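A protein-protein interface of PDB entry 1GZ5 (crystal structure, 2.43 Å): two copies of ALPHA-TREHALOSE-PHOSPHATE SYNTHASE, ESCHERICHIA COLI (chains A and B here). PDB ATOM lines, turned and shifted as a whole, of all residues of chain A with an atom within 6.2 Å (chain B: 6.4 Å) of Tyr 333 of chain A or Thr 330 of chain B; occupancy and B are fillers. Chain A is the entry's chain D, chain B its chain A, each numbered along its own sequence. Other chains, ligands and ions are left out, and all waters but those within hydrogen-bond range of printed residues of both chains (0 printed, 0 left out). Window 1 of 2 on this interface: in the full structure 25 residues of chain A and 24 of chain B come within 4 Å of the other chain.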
ATOM      1  N   ARG A 291      11.244   8.095  -9.486  1.00  0.00           N
ATOM      2  CA  ARG A 291      10.660   8.732 -10.635  1.00  0.00           C
ATOM      3  C   ARG A 291       9.271   8.179 -10.804  1.00  0.00           C
ATOM      4  O   ARG A 291       9.064   6.970 -10.719  1.00  0.00           O
ATOM      5  CB  ARG A 291      11.448   8.327 -11.823  1.00  0.00           C
ATOM      6  CG  ARG A 291      11.064   9.002 -13.085  1.00  0.00           C
ATOM      7  CD  ARG A 291      12.286   9.503 -13.723  1.00  0.00           C
ATOM      8  NE  ARG A 291      12.289   9.169 -15.119  1.00  0.00           N
ATOM      9  CZ  ARG A 291      13.328   9.360 -15.933  1.00  0.00           C
ATOM     10  NH1 ARG A 291      14.490   9.876 -15.501  1.00  0.00           N
ATOM     11  NH2 ARG A 291      13.196   9.015 -17.210  1.00  0.00           N
ATOM     12  N   TYR A 292       8.302   9.046 -11.030  1.00  0.00           N
ATOM     13  CA  TYR A 292       6.951   8.585 -11.285  1.00  0.00           C
ATOM     14  C   TYR A 292       6.647   9.000 -12.699  1.00  0.00           C
ATOM     15  O   TYR A 292       6.723  10.177 -13.041  1.00  0.00           O
ATOM     16  CB  TYR A 292       5.986   9.137 -10.227  1.00  0.00           C
ATOM     17  CG  TYR A 292       4.512   9.129 -10.574  1.00  0.00           C
ATOM     18  CD1 TYR A 292       3.943   8.109 -11.349  1.00  0.00           C
ATOM     19  CD2 TYR A 292       3.686  10.131 -10.113  1.00  0.00           C
ATOM     20  CE1 TYR A 292       2.605   8.103 -11.648  1.00  0.00           C
ATOM     21  CE2 TYR A 292       2.361  10.135 -10.421  1.00  0.00           C
ATOM     22  CZ  TYR A 292       1.817   9.115 -11.182  1.00  0.00           C
ATOM     23  OH  TYR A 292       0.473   9.162 -11.514  1.00  0.00           O
ATOM     24  N   THR A 293       6.371   8.015 -13.546  1.00  0.00           N
ATOM     25  CA  THR A 293       6.020   8.263 -14.905  1.00  0.00           C
ATOM     26  C   THR A 293       4.548   7.936 -15.070  1.00  0.00           C
ATOM     27  O   THR A 293       4.103   6.826 -14.733  1.00  0.00           O
ATOM     28  CB  THR A 293       6.835   7.357 -15.841  1.00  0.00           C
ATOM     29  OG1 THR A 293       8.215   7.689 -15.757  1.00  0.00           O
ATOM     30  CG2 THR A 293       6.537   7.647 -17.305  1.00  0.00           C
ATOM     31  N   GLN A 294       3.801   8.886 -15.632  1.00  0.00           N
ATOM     32  CA  GLN A 294       2.390   8.697 -15.891  1.00  0.00           C
ATOM     33  C   GLN A 294       2.094   8.823 -17.388  1.00  0.00           C
ATOM     34  O   GLN A 294       2.323   9.858 -18.011  1.00  0.00           O
ATOM     35  CB  GLN A 294       1.546   9.699 -15.107  1.00  0.00           C
ATOM     36  CG  GLN A 294       0.067   9.656 -15.552  1.00  0.00           C
ATOM     37  CD  GLN A 294      -0.640   8.401 -15.054  1.00  0.00           C
ATOM     38  OE1 GLN A 294      -0.729   8.159 -13.849  1.00  0.00           O
ATOM     39  NE2 GLN A 294      -1.122   7.588 -15.990  1.00  0.00           N
ATOM     40  N   ILE A 295       1.616   7.749 -17.976  1.00  0.00           N
ATOM     41  CA  ILE A 295       1.227   7.805 -19.365  1.00  0.00           C
ATOM     42  C   ILE A 295      -0.292   7.851 -19.426  1.00  0.00           C
ATOM     43  O   ILE A 295      -0.985   7.025 -18.827  1.00  0.00           O
ATOM     44  CB  ILE A 295       1.778   6.587 -20.058  1.00  0.00           C
ATOM     45  CG1 ILE A 295       3.311   6.670 -20.023  1.00  0.00           C
ATOM     46  CG2 ILE A 295       1.231   6.500 -21.502  1.00  0.00           C
ATOM     47  CD1 ILE A 295       3.988   5.622 -20.902  1.00  0.00           C
ATOM     48  N   ASN A 321       6.419  19.397 -10.429  1.00  0.00           N
ATOM     49  CA  ASN A 321       7.761  19.541 -10.908  1.00  0.00           C
ATOM     50  C   ASN A 321       8.335  20.889 -10.563  1.00  0.00           C
ATOM     51  O   ASN A 321       9.504  20.968 -10.217  1.00  0.00           O
ATOM     52  CB  ASN A 321       7.854  19.226 -12.394  1.00  0.00           C
ATOM     53  CG  ASN A 321       7.738  17.736 -12.667  1.00  0.00           C
ATOM     54  OD1 ASN A 321       8.181  16.906 -11.864  1.00  0.00           O
ATOM     55  ND2 ASN A 321       7.143  17.392 -13.751  1.00  0.00           N
ATOM     56  N   TRP A 329      16.874  16.674 -11.963  1.00  0.00           N
ATOM     57  CA  TRP A 329      15.930  15.651 -11.507  1.00  0.00           C
ATOM     58  C   TRP A 329      14.486  16.093 -11.642  1.00  0.00           C
ATOM     59  O   TRP A 329      14.051  16.971 -10.920  1.00  0.00           O
ATOM     60  CB  TRP A 329      16.183  15.270 -10.038  1.00  0.00           C
ATOM     61  CG  TRP A 329      15.248  14.184  -9.561  1.00  0.00           C
ATOM     62  CD1 TRP A 329      15.126  12.916 -10.078  1.00  0.00           C
ATOM     63  CD2 TRP A 329      14.301  14.265  -8.485  1.00  0.00           C
ATOM     64  NE1 TRP A 329      14.158  12.211  -9.398  1.00  0.00           N
ATOM     65  CE2 TRP A 329      13.635  13.003  -8.412  1.00  0.00           C
ATOM     66  CE3 TRP A 329      13.940  15.271  -7.568  1.00  0.00           C
ATOM     67  CZ2 TRP A 329      12.636  12.725  -7.465  1.00  0.00           C
ATOM     68  CZ3 TRP A 329      12.931  14.998  -6.628  1.00  0.00           C
ATOM     69  CH2 TRP A 329      12.282  13.734  -6.595  1.00  0.00           C
ATOM     70  N   THR A 330      13.767  15.495 -12.576  1.00  0.00           N
ATOM     71  CA  THR A 330      12.339  15.712 -12.738  1.00  0.00           C
ATOM     72  C   THR A 330      11.567  14.624 -12.015  1.00  0.00           C
ATOM     73  O   THR A 330      11.603  13.476 -12.418  1.00  0.00           O
ATOM     74  CB  THR A 330      12.017  15.662 -14.192  1.00  0.00           C
ATOM     75  OG1 THR A 330      12.762  16.707 -14.818  1.00  0.00           O
ATOM     76  CG2 THR A 330      10.559  16.094 -14.416  1.00  0.00           C
ATOM     77  N   PRO A 331      10.900  14.963 -10.919  1.00  0.00           N
ATOM     78  CA  PRO A 331      10.206  13.955 -10.113  1.00  0.00           C
ATOM     79  C   PRO A 331       9.114  13.196 -10.873  1.00  0.00           C
ATOM     80  O   PRO A 331       8.884  11.992 -10.570  1.00  0.00           O
ATOM     81  CB  PRO A 331       9.557  14.769  -8.987  1.00  0.00           C
ATOM     82  CG  PRO A 331       9.936  16.133  -9.163  1.00  0.00           C
ATOM     83  CD  PRO A 331      10.799  16.315 -10.351  1.00  0.00           C
ATOM     84  N   LEU A 332       8.463  13.865 -11.819  1.00  0.00           N
ATOM     85  CA  LEU A 332       7.242  13.373 -12.417  1.00  0.00           C
ATOM     86  C   LEU A 332       7.260  13.548 -13.925  1.00  0.00           C
ATOM     87  O   LEU A 332       7.408  14.641 -14.377  1.00  0.00           O
ATOM     88  CB  LEU A 332       6.062  14.169 -11.873  1.00  0.00           C
ATOM     89  CG  LEU A 332       4.689  13.543 -12.013  1.00  0.00           C
ATOM     90  CD1 LEU A 332       3.678  14.280 -11.149  1.00  0.00           C
ATOM     91  CD2 LEU A 332       4.267  13.599 -13.392  1.00  0.00           C
ATOM     92  N   TYR A 333       7.098  12.451 -14.669  1.00  0.00           N
ATOM     93  CA  TYR A 333       7.113  12.436 -16.128  1.00  0.00           C
ATOM     94  C   TYR A 333       5.676  12.193 -16.531  1.00  0.00           C
ATOM     95  O   TYR A 333       5.173  11.068 -16.400  1.00  0.00           O
ATOM     96  CB  TYR A 333       8.031  11.305 -16.664  1.00  0.00           C
ATOM     97  CG  TYR A 333       9.500  11.697 -16.699  1.00  0.00           C
ATOM     98  CD1 TYR A 333      10.185  12.045 -15.513  1.00  0.00           C
ATOM     99  CD2 TYR A 333      10.219  11.709 -17.896  1.00  0.00           C
ATOM    100  CE1 TYR A 333      11.513  12.437 -15.539  1.00  0.00           C
ATOM    101  CE2 TYR A 333      11.562  12.101 -17.937  1.00  0.00           C
ATOM    102  CZ  TYR A 333      12.199  12.473 -16.750  1.00  0.00           C
ATOM    103  OH  TYR A 333      13.531  12.844 -16.739  1.00  0.00           O
ATOM    104  N   TYR A 334       4.986  13.237 -16.979  1.00  0.00           N
ATOM    105  CA  TYR A 334       3.622  13.094 -17.446  1.00  0.00           C
ATOM    106  C   TYR A 334       3.613  13.128 -18.973  1.00  0.00           C
ATOM    107  O   TYR A 334       4.130  14.022 -19.580  1.00  0.00           O
ATOM    108  CB  TYR A 334       2.779  14.183 -16.837  1.00  0.00           C
ATOM    109  CG  TYR A 334       1.491  14.475 -17.565  1.00  0.00           C
ATOM    110  CD1 TYR A 334       0.455  13.537 -17.613  1.00  0.00           C
ATOM    111  CD2 TYR A 334       1.310  15.686 -18.202  1.00  0.00           C
ATOM    112  CE1 TYR A 334      -0.737  13.812 -18.293  1.00  0.00           C
ATOM    113  CE2 TYR A 334       0.132  15.960 -18.886  1.00  0.00           C
ATOM    114  CZ  TYR A 334      -0.883  15.002 -18.924  1.00  0.00           C
ATOM    115  OH  TYR A 334      -2.038  15.303 -19.620  1.00  0.00           O
ATOM    116  N   LEU A 335       3.116  12.058 -19.589  1.00  0.00           N
ATOM    117  CA  LEU A 335       3.090  11.957 -21.021  1.00  0.00           C
ATOM    118  C   LEU A 335       1.648  11.764 -21.478  1.00  0.00           C
ATOM    119  O   LEU A 335       1.004  10.760 -21.170  1.00  0.00           O
ATOM    120  CB  LEU A 335       3.995  10.829 -21.491  1.00  0.00           C
ATOM    121  CG  LEU A 335       5.486  10.832 -21.108  1.00  0.00           C
ATOM    122  CD1 LEU A 335       6.213   9.704 -21.830  1.00  0.00           C
ATOM    123  CD2 LEU A 335       6.139  12.124 -21.510  1.00  0.00           C
ATOM    124  N   TYR B 276       9.503  28.169 -27.273  1.00  0.00           N
ATOM    125  CA  TYR B 276      10.174  26.899 -27.144  1.00  0.00           C
ATOM    126  C   TYR B 276       9.379  25.789 -27.795  1.00  0.00           C
ATOM    127  O   TYR B 276       9.949  25.000 -28.526  1.00  0.00           O
ATOM    128  CB  TYR B 276      10.473  26.551 -25.706  1.00  0.00           C
ATOM    129  CG  TYR B 276      11.307  25.302 -25.531  1.00  0.00           C
ATOM    130  CD1 TYR B 276      12.562  25.194 -26.099  1.00  0.00           C
ATOM    131  CD2 TYR B 276      10.848  24.246 -24.786  1.00  0.00           C
ATOM    132  CE1 TYR B 276      13.328  24.060 -25.888  1.00  0.00           C
ATOM    133  CE2 TYR B 276      11.589  23.151 -24.594  1.00  0.00           C
ATOM    134  CZ  TYR B 276      12.829  23.044 -25.150  1.00  0.00           C
ATOM    135  OH  TYR B 276      13.601  21.906 -24.917  1.00  0.00           O
ATOM    136  N   ILE B 290      18.549  18.950 -26.589  1.00  0.00           N
ATOM    137  CA  ILE B 290      18.533  20.263 -25.981  1.00  0.00           C
ATOM    138  C   ILE B 290      17.620  20.193 -24.794  1.00  0.00           C
ATOM    139  O   ILE B 290      16.890  19.207 -24.622  1.00  0.00           O
ATOM    140  CB  ILE B 290      18.040  21.399 -26.967  1.00  0.00           C
ATOM    141  CG1 ILE B 290      16.536  21.231 -27.286  1.00  0.00           C
ATOM    142  CG2 ILE B 290      18.929  21.446 -28.243  1.00  0.00           C
ATOM    143  CD1 ILE B 290      15.925  22.389 -28.059  1.00  0.00           C
ATOM    144  N   ARG B 291      17.633  21.273 -24.017  1.00  0.00           N
ATOM    145  CA  ARG B 291      16.890  21.370 -22.763  1.00  0.00           C
ATOM    146  C   ARG B 291      16.690  22.813 -22.450  1.00  0.00           C
ATOM    147  O   ARG B 291      17.616  23.590 -22.521  1.00  0.00           O
ATOM    148  CB  ARG B 291      17.783  20.821 -21.708  1.00  0.00           C
ATOM    149  CG  ARG B 291      17.112  20.673 -20.386  1.00  0.00           C
ATOM    150  CD  ARG B 291      17.511  19.310 -19.878  1.00  0.00           C
ATOM    151  NE  ARG B 291      17.868  19.410 -18.511  1.00  0.00           N
ATOM    152  CZ  ARG B 291      18.232  18.393 -17.800  1.00  0.00           C
ATOM    153  NH1 ARG B 291      18.368  17.156 -18.352  1.00  0.00           N
ATOM    154  NH2 ARG B 291      18.514  18.637 -16.531  1.00  0.00           N
ATOM    155  N   TYR B 292      15.478  23.209 -22.146  1.00  0.00           N
ATOM    156  CA  TYR B 292      15.237  24.558 -21.742  1.00  0.00           C
ATOM    157  C   TYR B 292      14.894  24.491 -20.234  1.00  0.00           C
ATOM    158  O   TYR B 292      14.002  23.745 -19.813  1.00  0.00           O
ATOM    159  CB  TYR B 292      14.128  25.160 -22.632  1.00  0.00           C
ATOM    160  CG  TYR B 292      13.450  26.420 -22.104  1.00  0.00           C
ATOM    161  CD1 TYR B 292      14.136  27.381 -21.323  1.00  0.00           C
ATOM    162  CD2 TYR B 292      12.127  26.642 -22.358  1.00  0.00           C
ATOM    163  CE1 TYR B 292      13.470  28.524 -20.842  1.00  0.00           C
ATOM    164  CE2 TYR B 292      11.503  27.746 -21.885  1.00  0.00           C
ATOM    165  CZ  TYR B 292      12.167  28.683 -21.140  1.00  0.00           C
ATOM    166  OH  TYR B 292      11.426  29.756 -20.694  1.00  0.00           O
ATOM    167  N   ASN B 321       5.591  19.493 -21.873  1.00  0.00           N
ATOM    168  CA  ASN B 321       6.198  18.258 -21.548  1.00  0.00           C
ATOM    169  C   ASN B 321       5.312  17.100 -21.841  1.00  0.00           C
ATOM    170  O   ASN B 321       5.814  16.042 -22.289  1.00  0.00           O
ATOM    171  CB  ASN B 321       6.703  18.221 -20.093  1.00  0.00           C
ATOM    172  CG  ASN B 321       7.947  19.080 -19.887  1.00  0.00           C
ATOM    173  OD1 ASN B 321       8.792  19.170 -20.783  1.00  0.00           O
ATOM    174  ND2 ASN B 321       8.027  19.767 -18.755  1.00  0.00           N
ATOM    175  N   GLY B 325       7.519  15.457 -24.449  1.00  0.00           N
ATOM    176  CA  GLY B 325       8.386  14.641 -23.617  1.00  0.00           C
ATOM    177  C   GLY B 325       8.473  13.211 -24.112  1.00  0.00           C
ATOM    178  O   GLY B 325       7.633  12.739 -24.851  1.00  0.00           O
ATOM    179  N   GLN B 326       9.514  12.515 -23.705  1.00  0.00           N
ATOM    180  CA  GLN B 326       9.693  11.089 -23.988  1.00  0.00           C
ATOM    181  C   GLN B 326       9.970  10.429 -22.681  1.00  0.00           C
ATOM    182  O   GLN B 326      10.170  11.101 -21.699  1.00  0.00           O
ATOM    183  CB  GLN B 326      10.839  10.864 -24.951  1.00  0.00           C
ATOM    184  CG  GLN B 326      10.771  11.692 -26.226  1.00  0.00           C
ATOM    185  CD  GLN B 326      12.091  11.668 -27.007  1.00  0.00           C
ATOM    186  OE1 GLN B 326      13.049  11.058 -26.577  1.00  0.00           O
ATOM    187  NE2 GLN B 326      12.138  12.347 -28.130  1.00  0.00           N
ATOM    188  N   LEU B 327       9.966   9.118 -22.639  1.00  0.00           N
ATOM    189  CA  LEU B 327      10.310   8.418 -21.402  1.00  0.00           C
ATOM    190  C   LEU B 327      11.632   8.862 -20.780  1.00  0.00           C
ATOM    191  O   LEU B 327      11.744   8.886 -19.551  1.00  0.00           O
ATOM    192  CB  LEU B 327      10.289   6.907 -21.570  1.00  0.00           C
ATOM    193  CG  LEU B 327       8.901   6.317 -21.843  1.00  0.00           C
ATOM    194  CD1 LEU B 327       9.031   4.859 -22.298  1.00  0.00           C
ATOM    195  CD2 LEU B 327       7.953   6.438 -20.647  1.00  0.00           C
ATOM    196  N   GLY B 328      12.612   9.201 -21.624  1.00  0.00           N
ATOM    197  CA  GLY B 328      13.931   9.588 -21.153  1.00  0.00           C
ATOM    198  C   GLY B 328      14.355  10.981 -21.576  1.00  0.00           C
ATOM    199  O   GLY B 328      15.545  11.236 -21.776  1.00  0.00           O
ATOM    200  N   TRP B 329      13.395  11.900 -21.680  1.00  0.00           N
ATOM    201  CA  TRP B 329      13.726  13.252 -22.082  1.00  0.00           C
ATOM    202  C   TRP B 329      12.599  14.226 -21.724  1.00  0.00           C
ATOM    203  O   TRP B 329      11.493  14.165 -22.296  1.00  0.00           O
ATOM    204  CB  TRP B 329      14.035  13.330 -23.589  1.00  0.00           C
ATOM    205  CG  TRP B 329      14.432  14.730 -24.006  1.00  0.00           C
ATOM    206  CD1 TRP B 329      15.497  15.466 -23.525  1.00  0.00           C
ATOM    207  CD2 TRP B 329      13.744  15.595 -24.949  1.00  0.00           C
ATOM    208  NE1 TRP B 329      15.522  16.702 -24.137  1.00  0.00           N
ATOM    209  CE2 TRP B 329      14.475  16.812 -25.012  1.00  0.00           C
ATOM    210  CE3 TRP B 329      12.633  15.435 -25.794  1.00  0.00           C
ATOM    211  CZ2 TRP B 329      14.126  17.862 -25.866  1.00  0.00           C
ATOM    212  CZ3 TRP B 329      12.267  16.504 -26.640  1.00  0.00           C
ATOM    213  CH2 TRP B 329      13.017  17.699 -26.654  1.00  0.00           C
ATOM    214  N   THR B 330      12.875  15.102 -20.765  1.00  0.00           N
ATOM    215  CA  THR B 330      12.001  16.197 -20.447  1.00  0.00           C
ATOM    216  C   THR B 330      12.466  17.454 -21.154  1.00  0.00           C
ATOM    217  O   THR B 330      13.511  17.939 -20.868  1.00  0.00           O
ATOM    218  CB  THR B 330      12.027  16.413 -18.966  1.00  0.00           C
ATOM    219  OG1 THR B 330      11.485  15.260 -18.364  1.00  0.00           O
ATOM    220  CG2 THR B 330      10.962  17.466 -18.588  1.00  0.00           C
ATOM    221  N   PRO B 331      11.735  17.939 -22.124  1.00  0.00           N
ATOM    222  CA  PRO B 331      12.171  19.111 -22.885  1.00  0.00           C
ATOM    223  C   PRO B 331      12.335  20.389 -22.061  1.00  0.00           C
ATOM    224  O   PRO B 331      13.160  21.240 -22.399  1.00  0.00           O
ATOM    225  CB  PRO B 331      11.033  19.322 -23.926  1.00  0.00           C
ATOM    226  CG  PRO B 331      10.043  18.333 -23.691  1.00  0.00           C
ATOM    227  CD  PRO B 331      10.504  17.338 -22.641  1.00  0.00           C
ATOM    228  N   LEU B 332      11.498  20.544 -21.039  1.00  0.00           N
ATOM    229  CA  LEU B 332      11.367  21.783 -20.341  1.00  0.00           C
ATOM    230  C   LEU B 332      11.425  21.595 -18.820  1.00  0.00           C
ATOM    231  O   LEU B 332      10.608  20.881 -18.260  1.00  0.00           O
ATOM    232  CB  LEU B 332      10.040  22.399 -20.734  1.00  0.00           C
ATOM    233  CG  LEU B 332       9.874  23.914 -20.458  1.00  0.00           C
ATOM    234  CD1 LEU B 332       8.650  24.503 -21.097  1.00  0.00           C
ATOM    235  CD2 LEU B 332       9.802  24.151 -19.008  1.00  0.00           C
ATOM    236  N   TYR B 333      12.393  22.225 -18.151  1.00  0.00           N
ATOM    237  CA  TYR B 333      12.547  22.120 -16.696  1.00  0.00           C
ATOM    238  C   TYR B 333      12.064  23.449 -16.118  1.00  0.00           C
ATOM    239  O   TYR B 333      12.722  24.460 -16.285  1.00  0.00           O
ATOM    240  CB  TYR B 333      14.007  21.871 -16.336  1.00  0.00           C
ATOM    241  CG  TYR B 333      14.429  20.429 -16.453  1.00  0.00           C
ATOM    242  CD1 TYR B 333      14.361  19.754 -17.675  1.00  0.00           C
ATOM    243  CD2 TYR B 333      14.919  19.732 -15.346  1.00  0.00           C
ATOM    244  CE1 TYR B 333      14.723  18.387 -17.788  1.00  0.00           C
ATOM    245  CE2 TYR B 333      15.311  18.350 -15.438  1.00  0.00           C
ATOM    246  CZ  TYR B 333      15.192  17.701 -16.674  1.00  0.00           C
ATOM    247  OH  TYR B 333      15.549  16.381 -16.818  1.00  0.00           O
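OH of Tyr 333 of chain B lies close to OG1 of Thr 330 of chain A (3.4 Å). O of Leu 327 of chain B is in hydrogen-bond range of NH2 of Arg 291 of chain A, 2.8 Å away.
N of Tyr 333 of chain A lies within hydrogen-bond range of O of Tyr 292 of chain A. The side-chain amide nitrogen of Asn 321 of chain B is in hydrogen-bond range of the backbone carbonyl oxygen of Leu 332 of chain B, 2.9 Å away. N of Tyr 333 of chain B is in hydrogen-bond range of O of Tyr 292 of chain B, at 2.8 Å. The guanidinium group (NH1) of Arg 291 of chain A lies within hydrogen-bond range of the side-chain hydroxyl (OH) of Tyr 333 of chain A (3.4 Å). O of Gln 294 of chain A is in hydrogen-bond range of N of Leu 335 of chain A (2.8 Å). The backbone carbonyl oxygen (O) of Tyr 333 of chain A lies within hydrogen-bond range of the backbone NH (N) of Gln 294 of chain A, 2.7 Å away.
Among the printed residues, merely in contact across the chains: Thr 293 of chain A with Leu 327 of chain B (3.8 Å), Tyr 333 of chain A with Gln 326 of chain B (3.9 Å), Tyr 333 of chain A with Leu 327 of chain B (3.6 Å), Tyr 333 of chain A with Thr 330 of chain B (3.2 Å), Tyr 334 of chain A with Asn 321 of chain B (3.8 Å), Leu 335 of chain A with Gly 325 of chain B (3.7 Å), Leu 335 of chain A with Gln 326 of chain B (3.9 Å) and Leu 335 of chain A with Leu 327 of chain B (3.9 Å).
Printed residues of chain B within 4 Å of Arg 291 of chain A: Leu 327 (2.8 Å). Of the printed residues of chain B, Thr 330 of chain A touches Tyr 333 (3.1 Å). Tyr 333 of chain A touches just these residues of chain B: Gln 326, Leu 327 and Thr 330. Of the printed residues of chain B, Leu 335 of chain A touches Gly 325, Gln 326 and Leu 327. Of the printed residues of chain A, Gln 326 of chain B touches Tyr 333 (3.9 Å) and Leu 335 (3.9 Å). Of chain A, only Tyr 333 (3.2 Å) comes within 4 Å of Thr 330 of chain B. Of the printed residues of chain A, Tyr 333 of chain B touches Thr 330. The nearest residue of chain B that does not touch Tyr 333 of chain A is Tyr 333 of chain B (4.1 Å). The nearest printed residue of chain A that does not touch Gln 326 of chain B is Arg 291 of chain A (5.8 Å).
Of the 14 printed residues of chain B, 6 touch a printed residue of chain A. Hydrophobic or aromatic side chains of chain B within 4 Å of the printed part of chain A: Leu 327 and Tyr 333. Hydrophobic or aromatic side chains of chain A within 4 Å of the printed part of chain B: Tyr 333 and Leu 335. Among the printed residues, no Asp or Glu carboxylate lies within 4 Å of a Lys or Arg side-chain nitrogen of the other chain.
Thr 330 of chain A touches Tyr 333 of chain B, and with the chains exchanged Tyr 333 of chain A touches Thr 330 of chain B.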
